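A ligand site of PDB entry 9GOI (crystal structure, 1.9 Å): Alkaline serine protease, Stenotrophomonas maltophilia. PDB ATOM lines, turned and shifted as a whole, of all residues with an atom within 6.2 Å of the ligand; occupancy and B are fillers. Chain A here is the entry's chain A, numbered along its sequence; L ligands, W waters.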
ATOM      1  N   ASP A  42      29.263 -11.877   6.662  1.00  0.00           N
ATOM      2  CA  ASP A  42      29.239 -11.085   7.885  1.00  0.00           C
ATOM      3  C   ASP A  42      30.466 -11.409   8.738  1.00  0.00           C
ATOM      4  O   ASP A  42      31.457 -11.925   8.210  1.00  0.00           O
ATOM      5  CB  ASP A  42      27.911 -11.339   8.583  1.00  0.00           C
ATOM      6  CG  ASP A  42      27.322 -10.162   9.333  1.00  0.00           C
ATOM      7  OD1 ASP A  42      27.947  -9.736  10.332  1.00  0.00           O
ATOM      8  OD2 ASP A  42      26.218  -9.686   8.915  1.00  0.00           O
ATOM      9  N   THR A  43      30.353 -11.175  10.052  1.00  0.00           N
ATOM     10  CA  THR A  43      31.494 -11.283  10.970  1.00  0.00           C
ATOM     11  C   THR A  43      31.785 -12.731  11.318  1.00  0.00           C
ATOM     12  O   THR A  43      32.681 -12.955  12.140  1.00  0.00           O
ATOM     13  CB  THR A  43      31.295 -10.480  12.255  1.00  0.00           C
ATOM     14  OG1 THR A  43      30.266 -11.113  13.016  1.00  0.00           O
ATOM     15  CG2 THR A  43      30.965  -9.013  12.017  1.00  0.00           C
ATOM     16  N   ASP A  85      35.463  -9.306  16.779  1.00  0.00           N
ATOM     17  CA  ASP A  85      35.947  -8.176  16.008  1.00  0.00           C
ATOM     18  C   ASP A  85      36.246  -6.959  16.889  1.00  0.00           C
ATOM     19  O   ASP A  85      36.379  -5.855  16.361  1.00  0.00           O
ATOM     20  CB  ASP A  85      34.950  -7.842  14.889  1.00  0.00           C
ATOM     21  CG  ASP A  85      33.570  -7.433  15.363  1.00  0.00           C
ATOM     22  OD1 ASP A  85      33.399  -7.173  16.595  1.00  0.00           O
ATOM     23  OD2 ASP A  85      32.645  -7.391  14.500  1.00  0.00           O
ATOM     24  N   ASP A 101      33.665  -3.165  21.795  1.00  0.00           N
ATOM     25  CA  ASP A 101      33.569  -4.576  22.100  1.00  0.00           C
ATOM     26  C   ASP A 101      33.189  -5.377  20.856  1.00  0.00           C
ATOM     27  O   ASP A 101      32.707  -4.823  19.858  1.00  0.00           O
ATOM     28  CB  ASP A 101      32.574  -4.794  23.227  1.00  0.00           C
ATOM     29  CG  ASP A 101      32.986  -4.122  24.530  1.00  0.00           C
ATOM     30  OD1 ASP A 101      34.164  -4.242  24.887  1.00  0.00           O
ATOM     31  OD2 ASP A 101      32.124  -3.487  25.159  1.00  0.00           O
ATOM     32  N   SER A 103      31.207  -7.459  18.276  1.00  0.00           N
ATOM     33  CA  SER A 103      29.817  -7.229  17.889  1.00  0.00           C
ATOM     34  C   SER A 103      28.964  -8.506  17.978  1.00  0.00           C
ATOM     35  O   SER A 103      27.760  -8.425  18.270  1.00  0.00           O
ATOM     36  CB  SER A 103      29.740  -6.653  16.497  1.00  0.00           C
ATOM     37  OG  SER A 103      30.183  -7.599  15.520  1.00  0.00           O
ATOM     38  N   HIS A 105      27.957  -9.655  15.367  1.00  0.00           N
ATOM     39  CA  HIS A 105      26.952  -9.132  14.457  1.00  0.00           C
ATOM     40  C   HIS A 105      26.404 -10.244  13.570  1.00  0.00           C
ATOM     41  O   HIS A 105      25.207 -10.315  13.324  1.00  0.00           O
ATOM     42  CB  HIS A 105      27.581  -7.932  13.749  1.00  0.00           C
ATOM     43  CG  HIS A 105      26.771  -7.247  12.704  1.00  0.00           C
ATOM     44  ND1 HIS A 105      26.680  -7.741  11.417  1.00  0.00           N
ATOM     45  CD2 HIS A 105      26.100  -6.097  12.718  1.00  0.00           C
ATOM     46  CE1 HIS A 105      25.966  -6.911  10.682  1.00  0.00           C
ATOM     47  NE2 HIS A 105      25.587  -5.911  11.452  1.00  0.00           N
ATOM     48  N   LEU A 138      34.171 -10.385   7.595  1.00  0.00           N
ATOM     49  CA  LEU A 138      34.472  -9.215   8.392  1.00  0.00           C
ATOM     50  C   LEU A 138      35.143  -9.676   9.689  1.00  0.00           C
ATOM     51  O   LEU A 138      34.680 -10.626  10.306  1.00  0.00           O
ATOM     52  CB  LEU A 138      33.244  -8.381   8.760  1.00  0.00           C
ATOM     53  CG  LEU A 138      32.426  -7.836   7.594  1.00  0.00           C
ATOM     54  CD1 LEU A 138      31.168  -7.136   8.108  1.00  0.00           C
ATOM     55  CD2 LEU A 138      33.269  -6.864   6.762  1.00  0.00           C
ATOM     56  N   GLY A 139      36.171  -8.921  10.100  1.00  0.00           N
ATOM     57  CA  GLY A 139      36.812  -9.126  11.388  1.00  0.00           C
ATOM     58  C   GLY A 139      37.192  -7.808  12.041  1.00  0.00           C
ATOM     59  O   GLY A 139      36.422  -6.853  12.054  1.00  0.00           O
ATOM     60  N   CYS A 141      38.284  -4.342  12.562  1.00  0.00           N
ATOM     61  CA  CYS A 141      38.211  -3.149  11.728  1.00  0.00           C
ATOM     62  C   CYS A 141      37.558  -3.420  10.377  1.00  0.00           C
ATOM     63  O   CYS A 141      37.719  -2.612   9.475  1.00  0.00           O
ATOM     64  CB  CYS A 141      39.592  -2.517  11.518  1.00  0.00           C
ATOM     65  SG  CYS A 141      40.272  -1.820  13.048  1.00  0.00           S
ATOM     66  N   GLY A 142      36.820  -4.527  10.210  1.00  0.00           N
ATOM     67  CA  GLY A 142      36.084  -4.767   8.979  1.00  0.00           C
ATOM     68  C   GLY A 142      36.743  -5.835   8.104  1.00  0.00           C
ATOM     69  O   GLY A 142      37.150  -6.874   8.581  1.00  0.00           O
ATOM     70  N   GLY A 143      36.805  -5.573   6.785  1.00  0.00           N
ATOM     71  CA  GLY A 143      37.282  -6.577   5.847  1.00  0.00           C
ATOM     72  C   GLY A 143      37.784  -5.973   4.536  1.00  0.00           C
ATOM     73  O   GLY A 143      38.009  -4.773   4.424  1.00  0.00           O
ATOM     74  N   MET A 175      23.894  -9.377   2.748  1.00  0.00           N
ATOM     75  CA  MET A 175      25.033  -8.544   3.099  1.00  0.00           C
ATOM     76  C   MET A 175      24.615  -7.386   4.007  1.00  0.00           C
ATOM     77  O   MET A 175      24.257  -6.292   3.544  1.00  0.00           O
ATOM     78  CB  MET A 175      25.778  -8.023   1.867  1.00  0.00           C
ATOM     79  CG  MET A 175      26.554  -9.149   1.186  1.00  0.00           C
ATOM     80  SD  MET A 175      27.692  -8.604  -0.103  1.00  0.00           S
ATOM     81  CE  MET A 175      26.430  -8.468  -1.351  1.00  0.00           C
ATOM     82  N   SER A 176      24.751  -7.623   5.328  1.00  0.00           N
ATOM     83  CA  SER A 176      24.551  -6.568   6.315  1.00  0.00           C
ATOM     84  C   SER A 176      25.894  -5.857   6.560  1.00  0.00           C
ATOM     85  O   SER A 176      26.489  -5.919   7.647  1.00  0.00           O
ATOM     86  CB  SER A 176      23.929  -7.126   7.579  1.00  0.00           C
ATOM     87  OG  SER A 176      22.580  -7.533   7.381  1.00  0.00           O
ATOM     88  N   LEU A 177      26.385  -5.222   5.504  1.00  0.00           N
ATOM     89  CA  LEU A 177      27.749  -4.684   5.486  1.00  0.00           C
ATOM     90  C   LEU A 177      27.843  -3.691   4.333  1.00  0.00           C
ATOM     91  O   LEU A 177      27.077  -3.772   3.383  1.00  0.00           O
ATOM     92  CB  LEU A 177      28.846  -5.753   5.381  1.00  0.00           C
ATOM     93  CG  LEU A 177      28.914  -6.593   4.107  1.00  0.00           C
ATOM     94  CD1 LEU A 177      29.562  -5.895   2.908  1.00  0.00           C
ATOM     95  CD2 LEU A 177      29.634  -7.875   4.402  1.00  0.00           C
ATOM     96  N   GLY A 178      28.784  -2.743   4.455  1.00  0.00           N
ATOM     97  CA  GLY A 178      28.978  -1.800   3.369  1.00  0.00           C
ATOM     98  C   GLY A 178      29.926  -0.684   3.770  1.00  0.00           C
ATOM     99  O   GLY A 178      30.442  -0.677   4.878  1.00  0.00           O
ATOM    100  N   GLY A 179      30.099   0.265   2.849  1.00  0.00           N
ATOM    101  CA  GLY A 179      31.004   1.376   3.042  1.00  0.00           C
ATOM    102  C   GLY A 179      30.809   2.434   1.954  1.00  0.00           C
ATOM    103  O   GLY A 179      29.991   2.253   1.065  1.00  0.00           O
ATOM    104  N   ALA A 204      21.903  -4.255   3.091  1.00  0.00           N
ATOM    105  CA  ALA A 204      21.572  -3.140   3.951  1.00  0.00           C
ATOM    106  C   ALA A 204      21.834  -1.820   3.234  1.00  0.00           C
ATOM    107  O   ALA A 204      22.847  -1.700   2.560  1.00  0.00           O
ATOM    108  CB  ALA A 204      22.389  -3.225   5.235  1.00  0.00           C
ATOM    109  N   ALA A 205      20.911  -0.847   3.355  1.00  0.00           N
ATOM    110  CA  ALA A 205      21.089   0.432   2.675  1.00  0.00           C
ATOM    111  C   ALA A 205      22.232   1.242   3.259  1.00  0.00           C
ATOM    112  O   ALA A 205      22.780   2.084   2.534  1.00  0.00           O
ATOM    113  CB  ALA A 205      19.791   1.237   2.697  1.00  0.00           C
ATOM    114  N   GLY A 206      22.558   1.058   4.562  1.00  0.00           N
ATOM    115  CA  GLY A 206      23.470   1.959   5.246  1.00  0.00           C
ATOM    116  C   GLY A 206      22.757   2.813   6.292  1.00  0.00           C
ATOM    117  O   GLY A 206      21.543   3.006   6.216  1.00  0.00           O
ATOM    118  N   ASN A 207      23.556   3.336   7.237  1.00  0.00           N
ATOM    119  CA  ASN A 207      23.063   4.010   8.425  1.00  0.00           C
ATOM    120  C   ASN A 207      23.644   5.427   8.602  1.00  0.00           C
ATOM    121  O   ASN A 207      23.804   5.905   9.728  1.00  0.00           O
ATOM    122  CB  ASN A 207      23.396   3.194   9.670  1.00  0.00           C
ATOM    123  CG  ASN A 207      23.093   1.727   9.503  1.00  0.00           C
ATOM    124  OD1 ASN A 207      21.962   1.352   9.136  1.00  0.00           O
ATOM    125  ND2 ASN A 207      24.094   0.883   9.684  1.00  0.00           N
ATOM    126  N   PRO A 217      27.813  -2.334  -0.901  1.00  0.00           N
ATOM    127  CA  PRO A 217      27.048  -2.636  -2.107  1.00  0.00           C
ATOM    128  C   PRO A 217      25.643  -2.076  -2.263  1.00  0.00           C
ATOM    129  O   PRO A 217      24.918  -2.524  -3.143  1.00  0.00           O
ATOM    130  CB  PRO A 217      26.983  -4.175  -2.012  1.00  0.00           C
ATOM    131  CG  PRO A 217      26.880  -4.454  -0.524  1.00  0.00           C
ATOM    132  CD  PRO A 217      27.825  -3.447   0.059  1.00  0.00           C
ATOM    133  N   TYR A 238      18.616   6.890  11.321  1.00  0.00           N
ATOM    134  CA  TYR A 238      19.903   6.570  10.697  1.00  0.00           C
ATOM    135  C   TYR A 238      19.740   6.057   9.261  1.00  0.00           C
ATOM    136  O   TYR A 238      20.713   6.094   8.492  1.00  0.00           O
ATOM    137  CB  TYR A 238      20.645   5.544  11.568  1.00  0.00           C
ATOM    138  CG  TYR A 238      19.864   4.262  11.822  1.00  0.00           C
ATOM    139  CD1 TYR A 238      19.775   3.283  10.841  1.00  0.00           C
ATOM    140  CD2 TYR A 238      19.190   4.043  13.027  1.00  0.00           C
ATOM    141  CE1 TYR A 238      19.025   2.129  11.029  1.00  0.00           C
ATOM    142  CE2 TYR A 238      18.472   2.874  13.252  1.00  0.00           C
ATOM    143  CZ  TYR A 238      18.397   1.917  12.252  1.00  0.00           C
ATOM    144  OH  TYR A 238      17.660   0.773  12.414  1.00  0.00           O
ATOM    145  N   MET A 285      19.898  -5.160  18.786  1.00  0.00           N
ATOM    146  CA  MET A 285      20.740  -4.350  17.928  1.00  0.00           C
ATOM    147  C   MET A 285      19.829  -3.574  16.981  1.00  0.00           C
ATOM    148  O   MET A 285      18.763  -4.046  16.641  1.00  0.00           O
ATOM    149  CB  MET A 285      21.679  -5.239  17.100  1.00  0.00           C
ATOM    150  CG  MET A 285      22.788  -5.942  17.880  1.00  0.00           C
ATOM    151  SD  MET A 285      23.980  -6.760  16.784  1.00  0.00           S
ATOM    152  CE  MET A 285      24.675  -5.326  15.974  1.00  0.00           C
ATOM    153  N   GLY A 286      20.277  -2.395  16.556  1.00  0.00           N
ATOM    154  CA  GLY A 286      19.561  -1.613  15.570  1.00  0.00           C
ATOM    155  C   GLY A 286      20.426  -1.358  14.333  1.00  0.00           C
ATOM    156  O   GLY A 286      21.641  -1.156  14.429  1.00  0.00           O
ATOM    157  N   GLY A 287      19.808  -1.339  13.160  1.00  0.00           N
ATOM    158  CA  GLY A 287      20.503  -0.916  11.953  1.00  0.00           C
ATOM    159  C   GLY A 287      19.783  -1.409  10.697  1.00  0.00           C
ATOM    160  O   GLY A 287      18.931  -2.315  10.770  1.00  0.00           O
ATOM    161  N   THR A 288      20.177  -0.848   9.551  1.00  0.00           N
ATOM    162  CA  THR A 288      19.815  -1.476   8.271  1.00  0.00           C
ATOM    163  C   THR A 288      20.351  -2.915   8.233  1.00  0.00           C
ATOM    164  O   THR A 288      19.769  -3.768   7.548  1.00  0.00           O
ATOM    165  CB  THR A 288      20.220  -0.612   7.068  1.00  0.00           C
ATOM    166  OG1 THR A 288      21.621  -0.352   7.102  1.00  0.00           O
ATOM    167  CG2 THR A 288      19.434   0.687   6.998  1.00  0.00           C
ATOM    168  N   SER A 289      21.403  -3.221   9.016  1.00  0.00           N
ATOM    169  CA  SER A 289      21.926  -4.575   9.173  1.00  0.00           C
ATOM    170  C   SER A 289      20.848  -5.568   9.639  1.00  0.00           C
ATOM    171  O   SER A 289      20.923  -6.768   9.346  1.00  0.00           O
ATOM    172  CB  SER A 289      23.157  -4.605  10.123  1.00  0.00           C
ATOM    173  OG  SER A 289      24.222  -3.753   9.675  1.00  0.00           O
ATOM    174  N   MET A 290      19.911  -5.104  10.493  1.00  0.00           N
ATOM    175  CA  MET A 290      18.851  -5.931  11.054  1.00  0.00           C
ATOM    176  C   MET A 290      17.644  -6.014  10.098  1.00  0.00           C
ATOM    177  O   MET A 290      16.889  -6.995  10.124  1.00  0.00           O
ATOM    178  CB  MET A 290      18.386  -5.333  12.392  1.00  0.00           C
ATOM    179  CG  MET A 290      19.338  -5.530  13.556  1.00  0.00           C
ATOM    180  SD  MET A 290      20.973  -4.762  13.446  1.00  0.00           S
ATOM    181  CE  MET A 290      22.077  -6.145  13.097  1.00  0.00           C
HETATM  182  N1  LIG L   1      32.541  -1.676   7.067  1.00  0.00           N
HETATM  183  C1  LIG L   1      32.184  -2.419   8.127  1.00  0.00           C
HETATM  184  C2  LIG L   1      33.004  -2.538   9.230  1.00  0.00           C
HETATM  185  N2  LIG L   1      34.192  -1.930   9.300  1.00  0.00           N
HETATM  186  C3  LIG L   1      34.546  -1.200   8.233  1.00  0.00           C
HETATM  187  C4  LIG L   1      33.724  -1.063   7.144  1.00  0.00           C
HETATM  188  C5  LIG L   1      30.853  -3.114   8.082  1.00  0.00           C
HETATM  189  O1  LIG L   1      30.199  -3.123   7.049  1.00  0.00           O
HETATM  190  N3  LIG L   1      30.447  -3.655   9.221  1.00  0.00           N
HETATM  191  C6  LIG L   1      29.105  -4.222   9.396  1.00  0.00           C
HETATM  192  C7  LIG L   1      29.005  -5.182  10.613  1.00  0.00           C
HETATM  193  C8  LIG L   1      29.454  -4.638  11.937  1.00  0.00           C
HETATM  194  C9  LIG L   1      30.725  -4.949  12.458  1.00  0.00           C
HETATM  195  C10 LIG L   1      31.128  -4.459  13.680  1.00  0.00           C
HETATM  196  C11 LIG L   1      30.320  -3.624  14.400  1.00  0.00           C
HETATM  197  C12 LIG L   1      29.073  -3.288  13.901  1.00  0.00           C
HETATM  198  C13 LIG L   1      28.651  -3.778  12.669  1.00  0.00           C
HETATM  199  C14 LIG L   1      28.147  -3.038   9.519  1.00  0.00           C
HETATM  200  O2  LIG L   1      28.459  -1.917   9.945  1.00  0.00           O
HETATM  201  N4  LIG L   1      26.914  -3.292   9.103  1.00  0.00           N
HETATM  202  C15 LIG L   1      25.821  -2.317   9.205  1.00  0.00           C
HETATM  203  C16 LIG L   1      25.241  -2.047   7.804  1.00  0.00           C
HETATM  204  C17 LIG L   1      26.181  -1.461   6.777  1.00  0.00           C
HETATM  205  C18 LIG L   1      26.615  -0.044   7.061  1.00  0.00           C
HETATM  206  C19 LIG L   1      25.592  -1.547   5.378  1.00  0.00           C
HETATM  207  B1  LIG L   1      24.717  -2.505  10.312  1.00  0.00           B
HETATM  208  O3  LIG L   1      25.167  -2.996  11.510  1.00  0.00           O
HETATM  209  O4  LIG L   1      23.498  -1.889  10.299  1.00  0.00           O
HETATM  210  O   HOH W   1      23.549  -0.536  12.874  1.00  0.00           O
HETATM  211  O   HOH W   2      29.390  -0.118  13.996  1.00  0.00           O
HETATM  212  O   HOH W   3      24.296  -2.711  14.011  1.00  0.00           O
HETATM  213  O   HOH W   4      33.687  -6.749  11.983  1.00  0.00           O
HETATM  214  O   HOH W   5      30.785  -1.211  11.604  1.00  0.00           O
HETATM  215  O   HOH W   6      32.847  -1.970  12.746  1.00  0.00           O
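N of Ser 289 sits close to O4 of the ligand. The side-chain hydroxyl of Ser 289 is bonded to a boron (B1) of the ligand (1.5 Å). The side-chain amide nitrogen (ND2) of Asn 207 sits at hydrogen-bond distance from an oxygen (O4) of the ligand, 2.9 Å away. A ring nitrogen (NE2) of His 105 is in hydrogen-bond range of an oxygen (O3) of the ligand, 2.9 Å away. An oxygen (O1) of the ligand is in hydrogen-bond range of the backbone NH of Gly 178. A nitrogen (N4) of the ligand is in hydrogen-bond range of the backbone carbonyl oxygen (O) of Ser 176, at 3.0 Å.
OG of Ser 289 sits close to NE2 of His 105. The backbone carbonyl oxygen (O) of Ser 289 lies within hydrogen-bond range of the side-chain hydroxyl (OG) of Ser 176. OG1 of Thr 288 sits at hydrogen-bond distance from OD1 of Asn 207 (2.7 Å). N of His 105 lies close to OG of Ser 103. N of Gly 287 lies within hydrogen-bond range of OH of Tyr 238. The side-chain hydroxyl (OG1) of Thr 288 is in hydrogen-bond range of the backbone NH (N) of Gly 206 (3.1 Å). O of Met 175 lies within hydrogen-bond range of N of Ala 204 (3.1 Å). The backbone carbonyl oxygen of Asp 42 sits at hydrogen-bond distance from the backbone NH of Leu 138 (3.2 Å).
Merely in contact with the ligand: Leu 177, Asp 85, Gly 142, Gly 287, Thr 288, Cys 141, Ala 204, Leu 138 and Ser 103. Hydrophobic or aromatic side chains that line the ligand: His 105, Leu 138, Leu 177 and Ala 204. Within 4 Å of the ligand: Asp 85, Ser 103, His 105, Leu 138, Cys 141, Gly 142, Ser 176, Leu 177, Gly 178, Ala 204, Asn 207, Gly 287, Thr 288 and Ser 289.
Water W3 bridges O3 of the ligand and O of Gly 286. Water W1 bridges O of Gly 286 and O4 of the ligand. Water W4 lies within hydrogen-bond range of the backbone carbonyl oxygen (O) of Gly 139 (2.7 Å) and the side-chain carboxylate (OD2) of Asp 85 (2.8 Å).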
